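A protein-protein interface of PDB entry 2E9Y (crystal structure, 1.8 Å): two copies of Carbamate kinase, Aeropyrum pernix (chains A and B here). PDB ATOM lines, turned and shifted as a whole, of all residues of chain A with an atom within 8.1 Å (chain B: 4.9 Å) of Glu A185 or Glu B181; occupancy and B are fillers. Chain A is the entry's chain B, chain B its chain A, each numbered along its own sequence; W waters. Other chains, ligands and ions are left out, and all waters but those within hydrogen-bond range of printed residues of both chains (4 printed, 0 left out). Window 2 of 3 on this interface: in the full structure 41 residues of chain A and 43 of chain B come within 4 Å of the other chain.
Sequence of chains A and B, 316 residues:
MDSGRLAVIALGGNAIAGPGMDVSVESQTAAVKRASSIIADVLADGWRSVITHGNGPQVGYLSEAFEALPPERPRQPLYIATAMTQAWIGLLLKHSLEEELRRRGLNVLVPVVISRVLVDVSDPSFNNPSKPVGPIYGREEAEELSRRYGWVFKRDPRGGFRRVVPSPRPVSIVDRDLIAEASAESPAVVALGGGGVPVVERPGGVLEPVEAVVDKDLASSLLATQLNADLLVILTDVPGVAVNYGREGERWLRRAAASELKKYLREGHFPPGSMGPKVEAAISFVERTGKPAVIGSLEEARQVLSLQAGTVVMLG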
ATOM      1  N   ARG A  48       9.875  31.117  13.170  1.00  0.00           N
ATOM      2  CA  ARG A  48      10.440  30.372  12.059  1.00  0.00           C
ATOM      3  C   ARG A  48       9.353  30.168  11.018  1.00  0.00           C
ATOM      4  O   ARG A  48       8.173  30.107  11.331  1.00  0.00           O
ATOM      5  CB  ARG A  48      10.867  29.012  12.597  1.00  0.00           C
ATOM      6  CG  ARG A  48      12.141  29.090  13.433  1.00  0.00           C
ATOM      7  CD  ARG A  48      12.700  27.700  13.756  1.00  0.00           C
ATOM      8  NE  ARG A  48      13.427  27.155  12.605  1.00  0.00           N
ATOM      9  CZ  ARG A  48      14.682  27.595  12.403  1.00  0.00           C
ATOM     10  NH1 ARG A  48      15.214  28.487  13.221  1.00  0.00           N
ATOM     11  NH2 ARG A  48      15.396  27.110  11.384  1.00  0.00           N
ATOM     12  N   VAL A 108      21.502  34.824   6.692  1.00  0.00           N
ATOM     13  CA  VAL A 108      21.057  33.484   6.317  1.00  0.00           C
ATOM     14  C   VAL A 108      20.558  33.359   4.880  1.00  0.00           C
ATOM     15  O   VAL A 108      20.124  34.335   4.266  1.00  0.00           O
ATOM     16  CB  VAL A 108      19.929  33.005   7.253  1.00  0.00           C
ATOM     17  CG1 VAL A 108      20.415  32.996   8.691  1.00  0.00           C
ATOM     18  CG2 VAL A 108      18.716  33.909   7.109  1.00  0.00           C
ATOM     19  N   LEU A 109      20.630  32.141   4.350  1.00  0.00           N
ATOM     20  CA  LEU A 109      20.168  31.866   2.998  1.00  0.00           C
ATOM     21  C   LEU A 109      18.740  31.349   3.092  1.00  0.00           C
ATOM     22  O   LEU A 109      18.372  30.675   4.058  1.00  0.00           O
ATOM     23  CB  LEU A 109      21.060  30.819   2.317  1.00  0.00           C
ATOM     24  CG  LEU A 109      22.530  31.193   2.091  1.00  0.00           C
ATOM     25  CD1 LEU A 109      23.263  30.007   1.480  1.00  0.00           C
ATOM     26  CD2 LEU A 109      22.626  32.408   1.176  1.00  0.00           C
ATOM     27  N   PRO A 111      16.027  28.995   1.278  1.00  0.00           N
ATOM     28  CA  PRO A 111      15.826  27.987   0.237  1.00  0.00           C
ATOM     29  C   PRO A 111      14.438  28.082  -0.395  1.00  0.00           C
ATOM     30  O   PRO A 111      13.481  28.538   0.238  1.00  0.00           O
ATOM     31  CB  PRO A 111      16.019  26.674   0.990  1.00  0.00           C
ATOM     32  CG  PRO A 111      15.441  26.985   2.333  1.00  0.00           C
ATOM     33  CD  PRO A 111      15.982  28.387   2.622  1.00  0.00           C
ATOM     34  N   LEU A 178      11.199  17.408   2.494  1.00  0.00           N
ATOM     35  CA  LEU A 178      12.221  18.351   2.056  1.00  0.00           C
ATOM     36  C   LEU A 178      11.958  19.723   2.671  1.00  0.00           C
ATOM     37  O   LEU A 178      12.888  20.440   3.028  1.00  0.00           O
ATOM     38  CB  LEU A 178      12.234  18.456   0.531  1.00  0.00           C
ATOM     39  CG  LEU A 178      12.823  17.243  -0.194  1.00  0.00           C
ATOM     40  CD1 LEU A 178      12.702  17.424  -1.702  1.00  0.00           C
ATOM     41  CD2 LEU A 178      14.290  17.085   0.211  1.00  0.00           C
ATOM     42  N   ILE A 179      10.684  20.076   2.798  1.00  0.00           N
ATOM     43  CA  ILE A 179      10.305  21.357   3.380  1.00  0.00           C
ATOM     44  C   ILE A 179      10.659  21.367   4.871  1.00  0.00           C
ATOM     45  O   ILE A 179      11.186  22.352   5.387  1.00  0.00           O
ATOM     46  CB  ILE A 179       8.796  21.609   3.178  1.00  0.00           C
ATOM     47  CG1 ILE A 179       8.501  21.696   1.674  1.00  0.00           C
ATOM     48  CG2 ILE A 179       8.369  22.886   3.879  1.00  0.00           C
ATOM     49  CD1 ILE A 179       7.021  21.728   1.329  1.00  0.00           C
ATOM     50  N   ALA A 180      10.389  20.258   5.549  1.00  0.00           N
ATOM     51  CA  ALA A 180      10.702  20.142   6.972  1.00  0.00           C
ATOM     52  C   ALA A 180      12.215  20.225   7.191  1.00  0.00           C
ATOM     53  O   ALA A 180      12.682  20.870   8.130  1.00  0.00           O
ATOM     54  CB  ALA A 180      10.165  18.829   7.520  1.00  0.00           C
ATOM     55  N   GLU A 181      12.982  19.574   6.324  1.00  0.00           N
ATOM     56  CA  GLU A 181      14.434  19.601   6.448  1.00  0.00           C
ATOM     57  C   GLU A 181      14.977  21.014   6.225  1.00  0.00           C
ATOM     58  O   GLU A 181      15.875  21.463   6.940  1.00  0.00           O
ATOM     59  CB  GLU A 181      15.069  18.627   5.449  1.00  0.00           C
ATOM     60  CG  GLU A 181      14.652  17.173   5.670  1.00  0.00           C
ATOM     61  CD  GLU A 181      15.254  16.217   4.655  1.00  0.00           C
ATOM     62  OE1 GLU A 181      15.563  16.652   3.527  1.00  0.00           O
ATOM     63  OE2 GLU A 181      15.402  15.019   4.981  1.00  0.00           O
ATOM     64  N   ALA A 182      14.432  21.716   5.234  1.00  0.00           N
ATOM     65  CA  ALA A 182      14.881  23.075   4.948  1.00  0.00           C
ATOM     66  C   ALA A 182      14.584  23.982   6.138  1.00  0.00           C
ATOM     67  O   ALA A 182      15.401  24.821   6.516  1.00  0.00           O
ATOM     68  CB  ALA A 182      14.176  23.611   3.705  1.00  0.00           C
ATOM     69  N   SER A 183      13.404  23.796   6.720  1.00  0.00           N
ATOM     70  CA  SER A 183      12.957  24.595   7.854  1.00  0.00           C
ATOM     71  C   SER A 183      13.831  24.369   9.084  1.00  0.00           C
ATOM     72  O   SER A 183      14.012  25.272   9.895  1.00  0.00           O
ATOM     73  CB  SER A 183      11.499  24.262   8.181  1.00  0.00           C
ATOM     74  OG  SER A 183      11.018  25.058   9.251  1.00  0.00           O
ATOM     75  N   ALA A 184      14.369  23.163   9.220  1.00  0.00           N
ATOM     76  CA  ALA A 184      15.227  22.856  10.357  1.00  0.00           C
ATOM     77  C   ALA A 184      16.522  23.644  10.236  1.00  0.00           C
ATOM     78  O   ALA A 184      17.129  24.014  11.239  1.00  0.00           O
ATOM     79  CB  ALA A 184      15.528  21.361  10.403  1.00  0.00           C
ATOM     80  N   GLU A 185      16.929  23.914   8.999  1.00  0.00           N
ATOM     81  CA  GLU A 185      18.165  24.640   8.733  1.00  0.00           C
ATOM     82  C   GLU A 185      18.035  26.153   8.570  1.00  0.00           C
ATOM     83  O   GLU A 185      19.006  26.880   8.768  1.00  0.00           O
ATOM     84  CB  GLU A 185      18.844  24.062   7.487  1.00  0.00           C
ATOM     85  CG  GLU A 185      19.592  22.765   7.728  1.00  0.00           C
ATOM     86  CD  GLU A 185      20.730  22.940   8.717  1.00  0.00           C
ATOM     87  OE1 GLU A 185      21.605  23.799   8.471  1.00  0.00           O
ATOM     88  OE2 GLU A 185      20.748  22.221   9.736  1.00  0.00           O
ATOM     89  N   SER A 186      16.850  26.631   8.208  1.00  0.00           N
ATOM     90  CA  SER A 186      16.651  28.062   8.011  1.00  0.00           C
ATOM     91  C   SER A 186      15.308  28.560   8.541  1.00  0.00           C
ATOM     92  O   SER A 186      14.284  27.893   8.385  1.00  0.00           O
ATOM     93  CB  SER A 186      16.765  28.409   6.525  1.00  0.00           C
ATOM     94  OG  SER A 186      16.576  29.801   6.318  1.00  0.00           O
ATOM     95  N   PRO A 187      15.300  29.753   9.165  1.00  0.00           N
ATOM     96  CA  PRO A 187      14.096  30.371   9.730  1.00  0.00           C
ATOM     97  C   PRO A 187      13.114  30.859   8.668  1.00  0.00           C
ATOM     98  O   PRO A 187      11.976  31.217   8.975  1.00  0.00           O
ATOM     99  CB  PRO A 187      14.665  31.512  10.568  1.00  0.00           C
ATOM    100  CG  PRO A 187      15.857  31.936   9.766  1.00  0.00           C
ATOM    101  CD  PRO A 187      16.480  30.608   9.390  1.00  0.00           C
ATOM    102  N   ALA A 188      13.564  30.881   7.419  1.00  0.00           N
ATOM    103  CA  ALA A 188      12.719  31.317   6.318  1.00  0.00           C
ATOM    104  C   ALA A 188      12.880  30.343   5.161  1.00  0.00           C
ATOM    105  O   ALA A 188      13.982  30.137   4.655  1.00  0.00           O
ATOM    106  CB  ALA A 188      13.103  32.728   5.880  1.00  0.00           C
ATOM    107  N   VAL A 189      11.774  29.732   4.766  1.00  0.00           N
ATOM    108  CA  VAL A 189      11.774  28.781   3.666  1.00  0.00           C
ATOM    109  C   VAL A 189      10.609  29.147   2.757  1.00  0.00           C
ATOM    110  O   VAL A 189       9.537  29.492   3.236  1.00  0.00           O
ATOM    111  CB  VAL A 189      11.566  27.330   4.177  1.00  0.00           C
ATOM    112  CG1 VAL A 189      11.419  26.377   2.993  1.00  0.00           C
ATOM    113  CG2 VAL A 189      12.743  26.908   5.059  1.00  0.00           C
ATOM    114  N   ASP B 177      26.239  26.897   0.423  1.00  0.00           N
ATOM    115  CA  ASP B 177      25.796  26.329   1.697  1.00  0.00           C
ATOM    116  C   ASP B 177      24.487  25.542   1.603  1.00  0.00           C
ATOM    117  O   ASP B 177      24.356  24.489   2.226  1.00  0.00           O
ATOM    118  CB  ASP B 177      25.670  27.421   2.770  1.00  0.00           C
ATOM    119  CG  ASP B 177      27.023  27.951   3.227  1.00  0.00           C
ATOM    120  OD1 ASP B 177      28.047  27.297   2.943  1.00  0.00           O
ATOM    121  OD2 ASP B 177      27.064  29.013   3.883  1.00  0.00           O
ATOM    122  N   LEU B 178      23.515  26.039   0.837  1.00  0.00           N
ATOM    123  CA  LEU B 178      22.249  25.321   0.696  1.00  0.00           C
ATOM    124  C   LEU B 178      22.485  24.018  -0.049  1.00  0.00           C
ATOM    125  O   LEU B 178      21.857  23.003   0.234  1.00  0.00           O
ATOM    126  CB  LEU B 178      21.220  26.161  -0.067  1.00  0.00           C
ATOM    127  CG  LEU B 178      20.630  27.344   0.699  1.00  0.00           C
ATOM    128  CD1 LEU B 178      19.705  28.133  -0.222  1.00  0.00           C
ATOM    129  CD2 LEU B 178      19.874  26.842   1.924  1.00  0.00           C
ATOM    130  N   ILE B 179      23.398  24.048  -1.012  1.00  0.00           N
ATOM    131  CA  ILE B 179      23.701  22.848  -1.771  1.00  0.00           C
ATOM    132  C   ILE B 179      24.375  21.827  -0.850  1.00  0.00           C
ATOM    133  O   ILE B 179      24.055  20.638  -0.891  1.00  0.00           O
ATOM    134  CB  ILE B 179      24.617  23.173  -2.968  1.00  0.00           C
ATOM    135  CG1 ILE B 179      23.861  24.094  -3.940  1.00  0.00           C
ATOM    136  CG2 ILE B 179      25.039  21.892  -3.675  1.00  0.00           C
ATOM    137  CD1 ILE B 179      24.714  24.633  -5.082  1.00  0.00           C
ATOM    138  N   ALA B 180      25.294  22.296  -0.012  1.00  0.00           N
ATOM    139  CA  ALA B 180      25.994  21.405   0.915  1.00  0.00           C
ATOM    140  C   ALA B 180      25.016  20.780   1.907  1.00  0.00           C
ATOM    141  O   ALA B 180      25.095  19.589   2.209  1.00  0.00           O
ATOM    142  CB  ALA B 180      27.083  22.170   1.657  1.00  0.00           C
ATOM    143  N   GLU B 181      24.095  21.589   2.416  1.00  0.00           N
ATOM    144  CA  GLU B 181      23.103  21.102   3.365  1.00  0.00           C
ATOM    145  C   GLU B 181      22.215  20.048   2.709  1.00  0.00           C
ATOM    146  O   GLU B 181      21.907  19.015   3.310  1.00  0.00           O
ATOM    147  CB  GLU B 181      22.252  22.268   3.870  1.00  0.00           C
ATOM    148  CG  GLU B 181      22.986  23.180   4.844  1.00  0.00           C
ATOM    149  CD  GLU B 181      22.304  24.518   5.023  1.00  0.00           C
ATOM    150  OE1 GLU B 181      21.075  24.594   4.820  1.00  0.00           O
ATOM    151  OE2 GLU B 181      22.993  25.495   5.378  1.00  0.00           O
ATOM    152  N   ALA B 182      21.811  20.309   1.469  1.00  0.00           N
ATOM    153  CA  ALA B 182      20.964  19.372   0.741  1.00  0.00           C
ATOM    154  C   ALA B 182      21.696  18.053   0.542  1.00  0.00           C
ATOM    155  O   ALA B 182      21.099  16.982   0.649  1.00  0.00           O
ATOM    156  CB  ALA B 182      20.573  19.959  -0.613  1.00  0.00           C
ATOM    157  N   SER B 183      22.991  18.142   0.248  1.00  0.00           N
ATOM    158  CA  SER B 183      23.822  16.962   0.015  1.00  0.00           C
ATOM    159  C   SER B 183      23.977  16.116   1.278  1.00  0.00           C
ATOM    160  O   SER B 183      24.089  14.889   1.210  1.00  0.00           O
ATOM    161  CB  SER B 183      25.202  17.386  -0.491  1.00  0.00           C
ATOM    162  OG  SER B 183      25.934  16.270  -0.962  1.00  0.00           O
ATOM    163  N   ALA B 184      23.992  16.773   2.428  1.00  0.00           N
ATOM    164  CA  ALA B 184      24.120  16.059   3.689  1.00  0.00           C
ATOM    165  C   ALA B 184      22.856  15.239   3.937  1.00  0.00           C
ATOM    166  O   ALA B 184      22.905  14.177   4.556  1.00  0.00           O
ATOM    167  CB  ALA B 184      24.341  17.049   4.826  1.00  0.00           C
ATOM    168  N   GLU B 185      21.727  15.728   3.433  1.00  0.00           N
ATOM    169  CA  GLU B 185      20.448  15.053   3.626  1.00  0.00           C
ATOM    170  C   GLU B 185      20.045  14.061   2.534  1.00  0.00           C
ATOM    171  O   GLU B 185      19.245  13.161   2.786  1.00  0.00           O
ATOM    172  CB  GLU B 185      19.336  16.093   3.797  1.00  0.00           C
ATOM    173  CG  GLU B 185      19.449  16.931   5.060  1.00  0.00           C
ATOM    174  CD  GLU B 185      19.325  16.096   6.322  1.00  0.00           C
ATOM    175  OE1 GLU B 185      18.290  15.416   6.487  1.00  0.00           O
ATOM    176  OE2 GLU B 185      20.263  16.117   7.147  1.00  0.00           O
HETATM  177  O   HOH W   1      16.561  12.570   4.029  1.00  0.00           O
HETATM  178  O   HOH W   2      22.124  27.195   7.877  1.00  0.00           O
HETATM  179  O   HOH W   3      19.541  26.641   5.472  1.00  0.00           O
HETATM  180  O   HOH W   4      16.881  15.018   1.848  1.00  0.00           O
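Glu A185 touches one residue of chain B. Printed residues of chain A within 4 Å of Glu B181: Glu A185 (3.5 Å). No residue of chain A comes within 4 Å of Ala B180. No residue of chain A comes within 4 Å of Ala B182. Printed residues of chain A within 4 Å of Glu B185: Glu A181 (3.3 Å). Of the printed residues of chain A, Asp B177 touches Leu A109 (3.8 Å). The nearest printed residue of chain B that does not touch Glu A185 is Leu B178 (6.3 Å).
Glu A181 touches Glu B185, and with the chains exchanged Glu A185 touches Glu B181. Positions printed for both chains: 178, 179, 180, 181, 182, 183, 184 and 185.
Water W3 bridges the side-chain carboxylate (OE1) of Glu B181 (2.6 Å) and the backbone carbonyl oxygen (O) of Glu A185 (3.3 Å). Water W4 bridges OE1 of Glu A181 (2.7 Å) and O of Glu B185 (3.1 Å). Water W1 lies within hydrogen-bond range of OE2 of Glu A181 and O of Glu B185. Water W2 bridges OE2 of Glu B181 and O of Glu A185.
The backbone carbonyl oxygen (O) of Leu A109 lies within hydrogen-bond range of the side-chain hydroxyl (OG) of Ser A186.
The side-chain carboxylate of Glu B185 lies close to the side-chain carboxylate of Glu A181, at 3.3 Å.
Hydrophobic or aromatic side chains of chain B that line the printed part of chain A: Leu B178.
Among the printed residues, merely in contact across the chains: Glu A185 with Glu B181 (3.5 Å), Leu A109 with Asp B177 (3.8 Å), Leu A109 with Leu B178 (3.8 Å) and Pro A111 with Leu B178 (3.9 Å).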
